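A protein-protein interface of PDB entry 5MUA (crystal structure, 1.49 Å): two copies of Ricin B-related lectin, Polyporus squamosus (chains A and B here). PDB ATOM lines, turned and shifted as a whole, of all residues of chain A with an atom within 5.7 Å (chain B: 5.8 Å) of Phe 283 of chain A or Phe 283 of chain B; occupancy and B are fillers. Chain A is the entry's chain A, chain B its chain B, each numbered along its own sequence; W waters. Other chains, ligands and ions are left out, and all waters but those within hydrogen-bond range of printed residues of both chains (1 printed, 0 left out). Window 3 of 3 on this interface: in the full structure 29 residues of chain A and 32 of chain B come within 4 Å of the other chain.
N of Lys 171 of chain A is in hydrogen-bond range of O of Tyr 282 of chain A, at 3.2 Å. O of Gly 284 of chain A lies within hydrogen-bond range of N of Tyr 173 of chain A (3.0 Å). The backbone carbonyl oxygen (O) of Leu 285 of chain A lies within hydrogen-bond range of the backbone NH (N) of Leu 238 of chain A, 2.8 Å away. The backbone carbonyl oxygen of Tyr 282 of chain B is in hydrogen-bond range of the backbone NH of Lys 171 of chain B (3.0 Å). N of Tyr 173 of chain B sits at hydrogen-bond distance from O of Gly 284 of chain B (3.1 Å). The backbone NH of Phe 240 of chain B sits at hydrogen-bond distance from the backbone carbonyl oxygen of Phe 283 of chain B, at 3.1 Å.
Water W1 lies within hydrogen-bond range of O of Tyr 282 of chain A (2.7 Å) and OH of Tyr 173 of chain B (3.4 Å).
The side-chain hydroxyl (OH) of Tyr 173 of chain A lies within hydrogen-bond range of the side-chain hydroxyl (OH) of Tyr 173 of chain B (3.3 Å).
Phe 283 of chain A touches just these residues of chain B: Tyr 173 (3.7 Å) and Phe 283 (3.4 Å). Printed residues of chain B within 4 Å of Phe 240 of chain A: Leu 285. Printed residues of chain A within 4 Å of Leu 285 of chain B: Phe 240 (3.7 Å). Printed residues of chain B within 4 Å of Lys 171 of chain A: Tyr 173 (3.4 Å). Printed residues of chain A within 4 Å of Phe 240 of chain B: Leu 285 (3.8 Å). Phe 170 of chain A touches none of the printed residues of chain B. Ala 281 of chain B touches none of the printed residues of chain A. The nearest residue of chain A that does not touch Phe 283 of chain B is Leu 285 of chain A (4.1 Å). The nearest printed residue of chain A that does not touch Leu 285 of chain B is Leu 238 of chain A (4.03 Å).
Lys 171 of chain A touches Tyr 173 of chain B (CB to OH, 3.4 Å). OH of Tyr 173 of chain A touches CB of Lys 171 of chain B (3.3 Å). Tyr 173 of chain A touches Tyr 282 of chain B. Tyr 173 of chain A touches Phe 283 of chain B (CE2 to CD1, 3.8 Å). Phe 240 of chain A touches Leu 285 of chain B. Tyr 173 of chain B touches Tyr 282 of chain A. Phe 283 of chain A touches Tyr 173 of chain B. Phe 283 of chain B touches Phe 283 of chain A. CD1 of Leu 285 of chain A touches CE2 of Phe 240 of chain B, 3.8 Å away.
Lys 171 of chain A touches Tyr 173 of chain B, and with the chains exchanged Tyr 173 of chain A touches Lys 171 of chain B. Tyr 173 of chain A touches Tyr 282 of chain B, and with the chains exchanged Tyr 282 of chain A touches Tyr 173 of chain B. Tyr 173 of chain A touches Phe 283 of chain B, and with the chains exchanged Phe 283 of chain A touches Tyr 173 of chain B. Phe 240 of chain A touches Leu 285 of chain B, and with the chains exchanged Leu 285 of chain A touches Phe 240 of chain B. Positions printed for both chains: 170, 171, 172, 173, 238, 239, 240, 241, 281, 282, 283, 284 and 285.
Of the 13 printed residues of chain B, 6 touch a printed residue of chain A. Hydrophobic or aromatic side chains of chain A within 4 Å of the printed part of chain B: Tyr 173, Phe 240, Tyr 282, Phe 283 and Leu 285.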
ATOM      1  N   PHE A 170     -28.129   3.443 -15.644  1.00  0.00           N
ATOM      2  CA  PHE A 170     -27.574   3.707 -16.984  1.00  0.00           C
ATOM      3  C   PHE A 170     -28.548   3.430 -18.099  1.00  0.00           C
ATOM      4  O   PHE A 170     -29.237   2.406 -18.119  1.00  0.00           O
ATOM      5  CB  PHE A 170     -26.306   2.884 -17.216  1.00  0.00           C
ATOM      6  CG  PHE A 170     -25.640   3.098 -18.546  1.00  0.00           C
ATOM      7  CD1 PHE A 170     -24.833   4.195 -18.765  1.00  0.00           C
ATOM      8  CD2 PHE A 170     -25.738   2.153 -19.541  1.00  0.00           C
ATOM      9  CE1 PHE A 170     -24.180   4.382 -19.968  1.00  0.00           C
ATOM     10  CE2 PHE A 170     -25.071   2.311 -20.736  1.00  0.00           C
ATOM     11  CZ  PHE A 170     -24.298   3.421 -20.962  1.00  0.00           C
ATOM     12  N   LYS A 171     -28.558   4.366 -19.056  1.00  0.00           N
ATOM     13  CA  LYS A 171     -29.364   4.265 -20.266  1.00  0.00           C
ATOM     14  C   LYS A 171     -28.432   4.711 -21.418  1.00  0.00           C
ATOM     15  O   LYS A 171     -27.662   5.662 -21.265  1.00  0.00           O
ATOM     16  CB  LYS A 171     -30.552   5.266 -20.137  1.00  0.00           C
ATOM     17  CG  LYS A 171     -31.854   4.699 -19.514  1.00  0.00           C
ATOM     18  CD  LYS A 171     -32.514   3.584 -20.383  1.00  0.00           C
ATOM     19  CE  LYS A 171     -32.416   3.792 -21.922  1.00  0.00           C
ATOM     20  NZ  LYS A 171     -32.949   2.736 -22.824  1.00  0.00           N
ATOM     21  N   SER A 172     -28.530   4.037 -22.556  1.00  0.00           N
ATOM     22  CA  SER A 172     -27.742   4.335 -23.708  1.00  0.00           C
ATOM     23  C   SER A 172     -28.596   4.406 -24.969  1.00  0.00           C
ATOM     24  O   SER A 172     -29.684   3.848 -25.013  1.00  0.00           O
ATOM     25  CB  SER A 172     -26.664   3.287 -23.852  1.00  0.00           C
ATOM     26  OG  SER A 172     -27.242   2.018 -24.091  1.00  0.00           O
ATOM     27  N   TYR A 173     -28.101   5.156 -25.934  1.00  0.00           N
ATOM     28  CA  TYR A 173     -28.791   5.372 -27.194  1.00  0.00           C
ATOM     29  C   TYR A 173     -27.766   5.252 -28.312  1.00  0.00           C
ATOM     30  O   TYR A 173     -26.659   5.774 -28.173  1.00  0.00           O
ATOM     31  CB  TYR A 173     -29.356   6.781 -27.210  1.00  0.00           C
ATOM     32  CG  TYR A 173     -30.216   7.044 -25.988  1.00  0.00           C
ATOM     33  CD1 TYR A 173     -31.561   6.667 -25.952  1.00  0.00           C
ATOM     34  CD2 TYR A 173     -29.640   7.552 -24.843  1.00  0.00           C
ATOM     35  CE1 TYR A 173     -32.329   6.884 -24.810  1.00  0.00           C
ATOM     36  CE2 TYR A 173     -30.405   7.750 -23.694  1.00  0.00           C
ATOM     37  CZ  TYR A 173     -31.741   7.393 -23.701  1.00  0.00           C
ATOM     38  OH  TYR A 173     -32.446   7.581 -22.530  1.00  0.00           O
ATOM     39  N   LEU A 238     -19.896   8.830 -26.149  1.00  0.00           N
ATOM     40  CA  LEU A 238     -20.007   9.896 -25.147  1.00  0.00           C
ATOM     41  C   LEU A 238     -20.649   9.268 -23.900  1.00  0.00           C
ATOM     42  O   LEU A 238     -21.567   8.427 -24.002  1.00  0.00           O
ATOM     43  CB  LEU A 238     -20.923  11.035 -25.679  1.00  0.00           C
ATOM     44  CG  LEU A 238     -21.412  12.117 -24.713  1.00  0.00           C
ATOM     45  CD1 LEU A 238     -20.311  13.059 -24.432  1.00  0.00           C
ATOM     46  CD2 LEU A 238     -22.548  12.908 -25.351  1.00  0.00           C
ATOM     47  N   MET A 239     -20.156   9.634 -22.715  1.00  0.00           N
ATOM     48  CA  MET A 239     -20.734   9.213 -21.466  1.00  0.00           C
ATOM     49  C   MET A 239     -20.788  10.405 -20.505  1.00  0.00           C
ATOM     50  O   MET A 239     -19.884  11.259 -20.542  1.00  0.00           O
ATOM     51  CB  MET A 239     -19.948   8.125 -20.803  1.00  0.00           C
ATOM     52  CG  MET A 239     -20.400   6.748 -21.146  1.00  0.00           C
ATOM     53  SD  MET A 239     -19.128   5.587 -20.505  1.00  0.00           S
ATOM     54  CE  MET A 239     -19.919   4.145 -21.213  1.00  0.00           C
ATOM     55  N   PHE A 240     -21.834  10.399 -19.710  1.00  0.00           N
ATOM     56  CA  PHE A 240     -21.899  11.165 -18.467  1.00  0.00           C
ATOM     57  C   PHE A 240     -21.847  10.149 -17.354  1.00  0.00           C
ATOM     58  O   PHE A 240     -22.630   9.161 -17.348  1.00  0.00           O
ATOM     59  CB  PHE A 240     -23.133  12.042 -18.310  1.00  0.00           C
ATOM     60  CG  PHE A 240     -23.250  13.226 -19.294  1.00  0.00           C
ATOM     61  CD1 PHE A 240     -22.295  13.567 -20.239  1.00  0.00           C
ATOM     62  CD2 PHE A 240     -24.306  14.106 -19.129  1.00  0.00           C
ATOM     63  CE1 PHE A 240     -22.391  14.640 -21.061  1.00  0.00           C
ATOM     64  CE2 PHE A 240     -24.433  15.194 -19.990  1.00  0.00           C
ATOM     65  CZ  PHE A 240     -23.490  15.468 -20.961  1.00  0.00           C
ATOM     66  N   GLY A 241     -21.032  10.450 -16.345  1.00  0.00           N
ATOM     67  CA  GLY A 241     -20.939   9.556 -15.177  1.00  0.00           C
ATOM     68  C   GLY A 241     -20.664  10.261 -13.899  1.00  0.00           C
ATOM     69  O   GLY A 241     -20.284  11.400 -13.925  1.00  0.00           O
ATOM     70  N   ALA A 281     -21.021   5.462 -15.303  1.00  0.00           N
ATOM     71  CA  ALA A 281     -21.810   6.125 -16.323  1.00  0.00           C
ATOM     72  C   ALA A 281     -23.283   6.006 -16.060  1.00  0.00           C
ATOM     73  O   ALA A 281     -23.800   4.917 -15.771  1.00  0.00           O
ATOM     74  CB  ALA A 281     -21.476   5.552 -17.711  1.00  0.00           C
ATOM     75  N   TYR A 282     -24.005   7.127 -16.198  1.00  0.00           N
ATOM     76  CA  TYR A 282     -25.478   7.103 -16.172  1.00  0.00           C
ATOM     77  C   TYR A 282     -26.130   7.337 -17.551  1.00  0.00           C
ATOM     78  O   TYR A 282     -27.309   6.994 -17.744  1.00  0.00           O
ATOM     79  CB  TYR A 282     -26.057   7.993 -15.115  1.00  0.00           C
ATOM     80  CG  TYR A 282     -25.724   9.434 -15.229  1.00  0.00           C
ATOM     81  CD1 TYR A 282     -26.480  10.323 -16.083  1.00  0.00           C
ATOM     82  CD2 TYR A 282     -24.676   9.982 -14.490  1.00  0.00           C
ATOM     83  CE1 TYR A 282     -26.161  11.691 -16.169  1.00  0.00           C
ATOM     84  CE2 TYR A 282     -24.359  11.347 -14.574  1.00  0.00           C
ATOM     85  CZ  TYR A 282     -25.107  12.198 -15.396  1.00  0.00           C
ATOM     86  OH  TYR A 282     -24.760  13.523 -15.421  1.00  0.00           O
ATOM     87  N   PHE A 283     -25.312   7.788 -18.504  1.00  0.00           N
ATOM     88  CA  PHE A 283     -25.749   8.100 -19.838  1.00  0.00           C
ATOM     89  C   PHE A 283     -24.681   7.753 -20.858  1.00  0.00           C
ATOM     90  O   PHE A 283     -23.501   8.136 -20.686  1.00  0.00           O
ATOM     91  CB  PHE A 283     -26.117   9.599 -19.910  1.00  0.00           C
ATOM     92  CG  PHE A 283     -26.137  10.174 -21.289  1.00  0.00           C
ATOM     93  CD1 PHE A 283     -26.988   9.686 -22.242  1.00  0.00           C
ATOM     94  CD2 PHE A 283     -25.362  11.278 -21.585  1.00  0.00           C
ATOM     95  CE1 PHE A 283     -26.973  10.203 -23.519  1.00  0.00           C
ATOM     96  CE2 PHE A 283     -25.362  11.822 -22.845  1.00  0.00           C
ATOM     97  CZ  PHE A 283     -26.172  11.299 -23.809  1.00  0.00           C
ATOM     98  N   GLY A 284     -25.074   7.028 -21.895  1.00  0.00           N
ATOM     99  CA  GLY A 284     -24.162   6.706 -22.970  1.00  0.00           C
ATOM    100  C   GLY A 284     -24.760   7.014 -24.343  1.00  0.00           C
ATOM    101  O   GLY A 284     -25.956   6.716 -24.570  1.00  0.00           O
ATOM    102  N   LEU A 285     -23.945   7.558 -25.246  1.00  0.00           N
ATOM    103  CA  LEU A 285     -24.409   7.865 -26.611  1.00  0.00           C
ATOM    104  C   LEU A 285     -23.320   7.399 -27.592  1.00  0.00           C
ATOM    105  O   LEU A 285     -22.092   7.700 -27.371  1.00  0.00           O
ATOM    106  CB  LEU A 285     -24.613   9.360 -26.756  1.00  0.00           C
ATOM    107  CG  LEU A 285     -24.970   9.851 -28.126  1.00  0.00           C
ATOM    108  CD1 LEU A 285     -26.362   9.364 -28.468  1.00  0.00           C
ATOM    109  CD2 LEU A 285     -24.949  11.380 -28.117  1.00  0.00           C
ATOM    110  N   PHE B 170     -39.364   9.242 -22.895  1.00  0.00           N
ATOM    111  CA  PHE B 170     -38.360  10.289 -23.086  1.00  0.00           C
ATOM    112  C   PHE B 170     -37.483  10.383 -21.858  1.00  0.00           C
ATOM    113  O   PHE B 170     -37.983  10.407 -20.736  1.00  0.00           O
ATOM    114  CB  PHE B 170     -39.026  11.641 -23.193  1.00  0.00           C
ATOM    115  CG  PHE B 170     -38.072  12.790 -23.385  1.00  0.00           C
ATOM    116  CD1 PHE B 170     -37.400  12.922 -24.554  1.00  0.00           C
ATOM    117  CD2 PHE B 170     -37.926  13.755 -22.418  1.00  0.00           C
ATOM    118  CE1 PHE B 170     -36.506  13.966 -24.781  1.00  0.00           C
ATOM    119  CE2 PHE B 170     -37.113  14.825 -22.645  1.00  0.00           C
ATOM    120  CZ  PHE B 170     -36.375  14.938 -23.825  1.00  0.00           C
ATOM    121  N   LYS B 171     -36.182  10.420 -22.069  1.00  0.00           N
ATOM    122  CA  LYS B 171     -35.205  10.796 -21.028  1.00  0.00           C
ATOM    123  C   LYS B 171     -34.297  11.894 -21.535  1.00  0.00           C
ATOM    124  O   LYS B 171     -33.895  11.899 -22.698  1.00  0.00           O
ATOM    125  CB  LYS B 171     -34.309   9.626 -20.680  1.00  0.00           C
ATOM    126  CG  LYS B 171     -34.984   8.308 -20.296  1.00  0.00           C
ATOM    127  CD  LYS B 171     -35.511   8.275 -18.869  1.00  0.00           C
ATOM    128  CE  LYS B 171     -36.069   6.893 -18.501  1.00  0.00           C
ATOM    129  NZ  LYS B 171     -37.515   6.826 -18.854  1.00  0.00           N
ATOM    130  N   SER B 172     -33.959  12.818 -20.653  1.00  0.00           N
ATOM    131  CA  SER B 172     -33.078  13.862 -20.985  1.00  0.00           C
ATOM    132  C   SER B 172     -32.002  13.979 -19.902  1.00  0.00           C
ATOM    133  O   SER B 172     -32.179  13.482 -18.766  1.00  0.00           O
ATOM    134  CB  SER B 172     -33.846  15.165 -21.118  1.00  0.00           C
ATOM    135  OG  SER B 172     -34.526  15.444 -19.924  1.00  0.00           O
ATOM    136  N   TYR B 173     -30.928  14.660 -20.295  1.00  0.00           N
ATOM    137  CA  TYR B 173     -29.718  14.819 -19.488  1.00  0.00           C
ATOM    138  C   TYR B 173     -29.249  16.255 -19.598  1.00  0.00           C
ATOM    139  O   TYR B 173     -29.199  16.802 -20.693  1.00  0.00           O
ATOM    140  CB  TYR B 173     -28.696  13.852 -20.025  1.00  0.00           C
ATOM    141  CG  TYR B 173     -29.196  12.408 -19.981  1.00  0.00           C
ATOM    142  CD1 TYR B 173     -29.188  11.675 -18.783  1.00  0.00           C
ATOM    143  CD2 TYR B 173     -29.789  11.851 -21.075  1.00  0.00           C
ATOM    144  CE1 TYR B 173     -29.664  10.386 -18.738  1.00  0.00           C
ATOM    145  CE2 TYR B 173     -30.319  10.587 -21.026  1.00  0.00           C
ATOM    146  CZ  TYR B 173     -30.241   9.871 -19.857  1.00  0.00           C
ATOM    147  OH  TYR B 173     -30.767   8.607 -19.848  1.00  0.00           O
ATOM    148  N   LEU B 238     -29.977  18.636 -28.254  1.00  0.00           N
ATOM    149  CA  LEU B 238     -29.954  17.457 -29.151  1.00  0.00           C
ATOM    150  C   LEU B 238     -31.168  16.601 -28.811  1.00  0.00           C
ATOM    151  O   LEU B 238     -31.465  16.406 -27.607  1.00  0.00           O
ATOM    152  CB  LEU B 238     -28.677  16.653 -28.975  1.00  0.00           C
ATOM    153  CG  LEU B 238     -28.543  15.337 -29.756  1.00  0.00           C
ATOM    154  CD1 LEU B 238     -28.597  15.630 -31.250  1.00  0.00           C
ATOM    155  CD2 LEU B 238     -27.203  14.739 -29.455  1.00  0.00           C
ATOM    156  N   MET B 239     -31.897  16.132 -29.845  1.00  0.00           N
ATOM    157  CA  MET B 239     -32.996  15.211 -29.633  1.00  0.00           C
ATOM    158  C   MET B 239     -32.879  14.064 -30.671  1.00  0.00           C
ATOM    159  O   MET B 239     -32.455  14.279 -31.761  1.00  0.00           O
ATOM    160  CB  MET B 239     -34.368  15.919 -29.832  1.00  0.00           C
ATOM    161  CG  MET B 239     -35.083  16.127 -28.552  1.00  0.00           C
ATOM    162  SD  MET B 239     -36.551  17.064 -28.981  1.00  0.00           S
ATOM    163  CE  MET B 239     -36.788  17.610 -27.299  1.00  0.00           C
ATOM    164  N   PHE B 240     -33.169  12.853 -30.238  1.00  0.00           N
ATOM    165  CA  PHE B 240     -33.480  11.726 -31.109  1.00  0.00           C
ATOM    166  C   PHE B 240     -34.963  11.452 -30.892  1.00  0.00           C
ATOM    167  O   PHE B 240     -35.455  11.309 -29.741  1.00  0.00           O
ATOM    168  CB  PHE B 240     -32.712  10.464 -30.681  1.00  0.00           C
ATOM    169  CG  PHE B 240     -31.247  10.466 -30.957  1.00  0.00           C
ATOM    170  CD1 PHE B 240     -30.555  11.540 -31.513  1.00  0.00           C
ATOM    171  CD2 PHE B 240     -30.545   9.275 -30.720  1.00  0.00           C
ATOM    172  CE1 PHE B 240     -29.206  11.470 -31.765  1.00  0.00           C
ATOM    173  CE2 PHE B 240     -29.175   9.194 -30.991  1.00  0.00           C
ATOM    174  CZ  PHE B 240     -28.515  10.302 -31.501  1.00  0.00           C
ATOM    175  N   GLY B 241     -35.688  11.369 -31.992  1.00  0.00           N
ATOM    176  CA  GLY B 241     -37.100  11.046 -31.921  1.00  0.00           C
ATOM    177  C   GLY B 241     -37.541  10.168 -33.075  1.00  0.00           C
ATOM    178  O   GLY B 241     -36.758   9.870 -33.981  1.00  0.00           O
ATOM    179  N   ALA B 281     -39.800  12.725 -29.310  1.00  0.00           N
ATOM    180  CA  ALA B 281     -38.485  12.463 -28.734  1.00  0.00           C
ATOM    181  C   ALA B 281     -38.416  11.354 -27.698  1.00  0.00           C
ATOM    182  O   ALA B 281     -39.289  11.221 -26.835  1.00  0.00           O
ATOM    183  CB  ALA B 281     -37.856  13.757 -28.216  1.00  0.00           C
ATOM    184  N   TYR B 282     -37.391  10.512 -27.824  1.00  0.00           N
ATOM    185  CA  TYR B 282     -37.062   9.567 -26.781  1.00  0.00           C
ATOM    186  C   TYR B 282     -35.831   9.923 -26.004  1.00  0.00           C
ATOM    187  O   TYR B 282     -35.618   9.413 -24.880  1.00  0.00           O
ATOM    188  CB  TYR B 282     -37.017   8.132 -27.283  1.00  0.00           C
ATOM    189  CG  TYR B 282     -36.055   7.870 -28.405  1.00  0.00           C
ATOM    190  CD1 TYR B 282     -34.698   7.527 -28.145  1.00  0.00           C
ATOM    191  CD2 TYR B 282     -36.486   7.857 -29.732  1.00  0.00           C
ATOM    192  CE1 TYR B 282     -33.817   7.298 -29.168  1.00  0.00           C
ATOM    193  CE2 TYR B 282     -35.577   7.600 -30.761  1.00  0.00           C
ATOM    194  CZ  TYR B 282     -34.246   7.276 -30.463  1.00  0.00           C
ATOM    195  OH  TYR B 282     -33.346   7.024 -31.475  1.00  0.00           O
ATOM    196  N   PHE B 283     -35.011  10.815 -26.553  1.00  0.00           N
ATOM    197  CA  PHE B 283     -33.759  11.207 -25.958  1.00  0.00           C
ATOM    198  C   PHE B 283     -33.541  12.712 -26.174  1.00  0.00           C
ATOM    199  O   PHE B 283     -33.735  13.229 -27.262  1.00  0.00           O
ATOM    200  CB  PHE B 283     -32.605  10.376 -26.523  1.00  0.00           C
ATOM    201  CG  PHE B 283     -31.283  11.011 -26.392  1.00  0.00           C
ATOM    202  CD1 PHE B 283     -30.728  11.216 -25.156  1.00  0.00           C
ATOM    203  CD2 PHE B 283     -30.576  11.417 -27.513  1.00  0.00           C
ATOM    204  CE1 PHE B 283     -29.493  11.838 -25.029  1.00  0.00           C
ATOM    205  CE2 PHE B 283     -29.326  12.021 -27.383  1.00  0.00           C
ATOM    206  CZ  PHE B 283     -28.810  12.273 -26.125  1.00  0.00           C
ATOM    207  N   GLY B 284     -33.176  13.404 -25.118  1.00  0.00           N
ATOM    208  CA  GLY B 284     -32.681  14.759 -25.223  1.00  0.00           C
ATOM    209  C   GLY B 284     -31.435  15.064 -24.412  1.00  0.00           C
ATOM    210  O   GLY B 284     -31.243  14.527 -23.343  1.00  0.00           O
ATOM    211  N   LEU B 285     -30.585  15.916 -24.932  1.00  0.00           N
ATOM    212  CA  LEU B 285     -29.360  16.343 -24.250  1.00  0.00           C
ATOM    213  C   LEU B 285     -29.272  17.851 -24.370  1.00  0.00           C
ATOM    214  O   LEU B 285     -29.485  18.366 -25.451  1.00  0.00           O
ATOM    215  CB  LEU B 285     -28.118  15.689 -24.887  1.00  0.00           C
ATOM    216  CG  LEU B 285     -26.746  16.160 -24.431  1.00  0.00           C
ATOM    217  CD1 LEU B 285     -26.579  15.746 -22.990  1.00  0.00           C
ATOM    218  CD2 LEU B 285     -25.576  15.572 -25.235  1.00  0.00           C
HETATM  219  O   HOH W   1     -29.777   7.471 -16.855  1.00  0.00           O
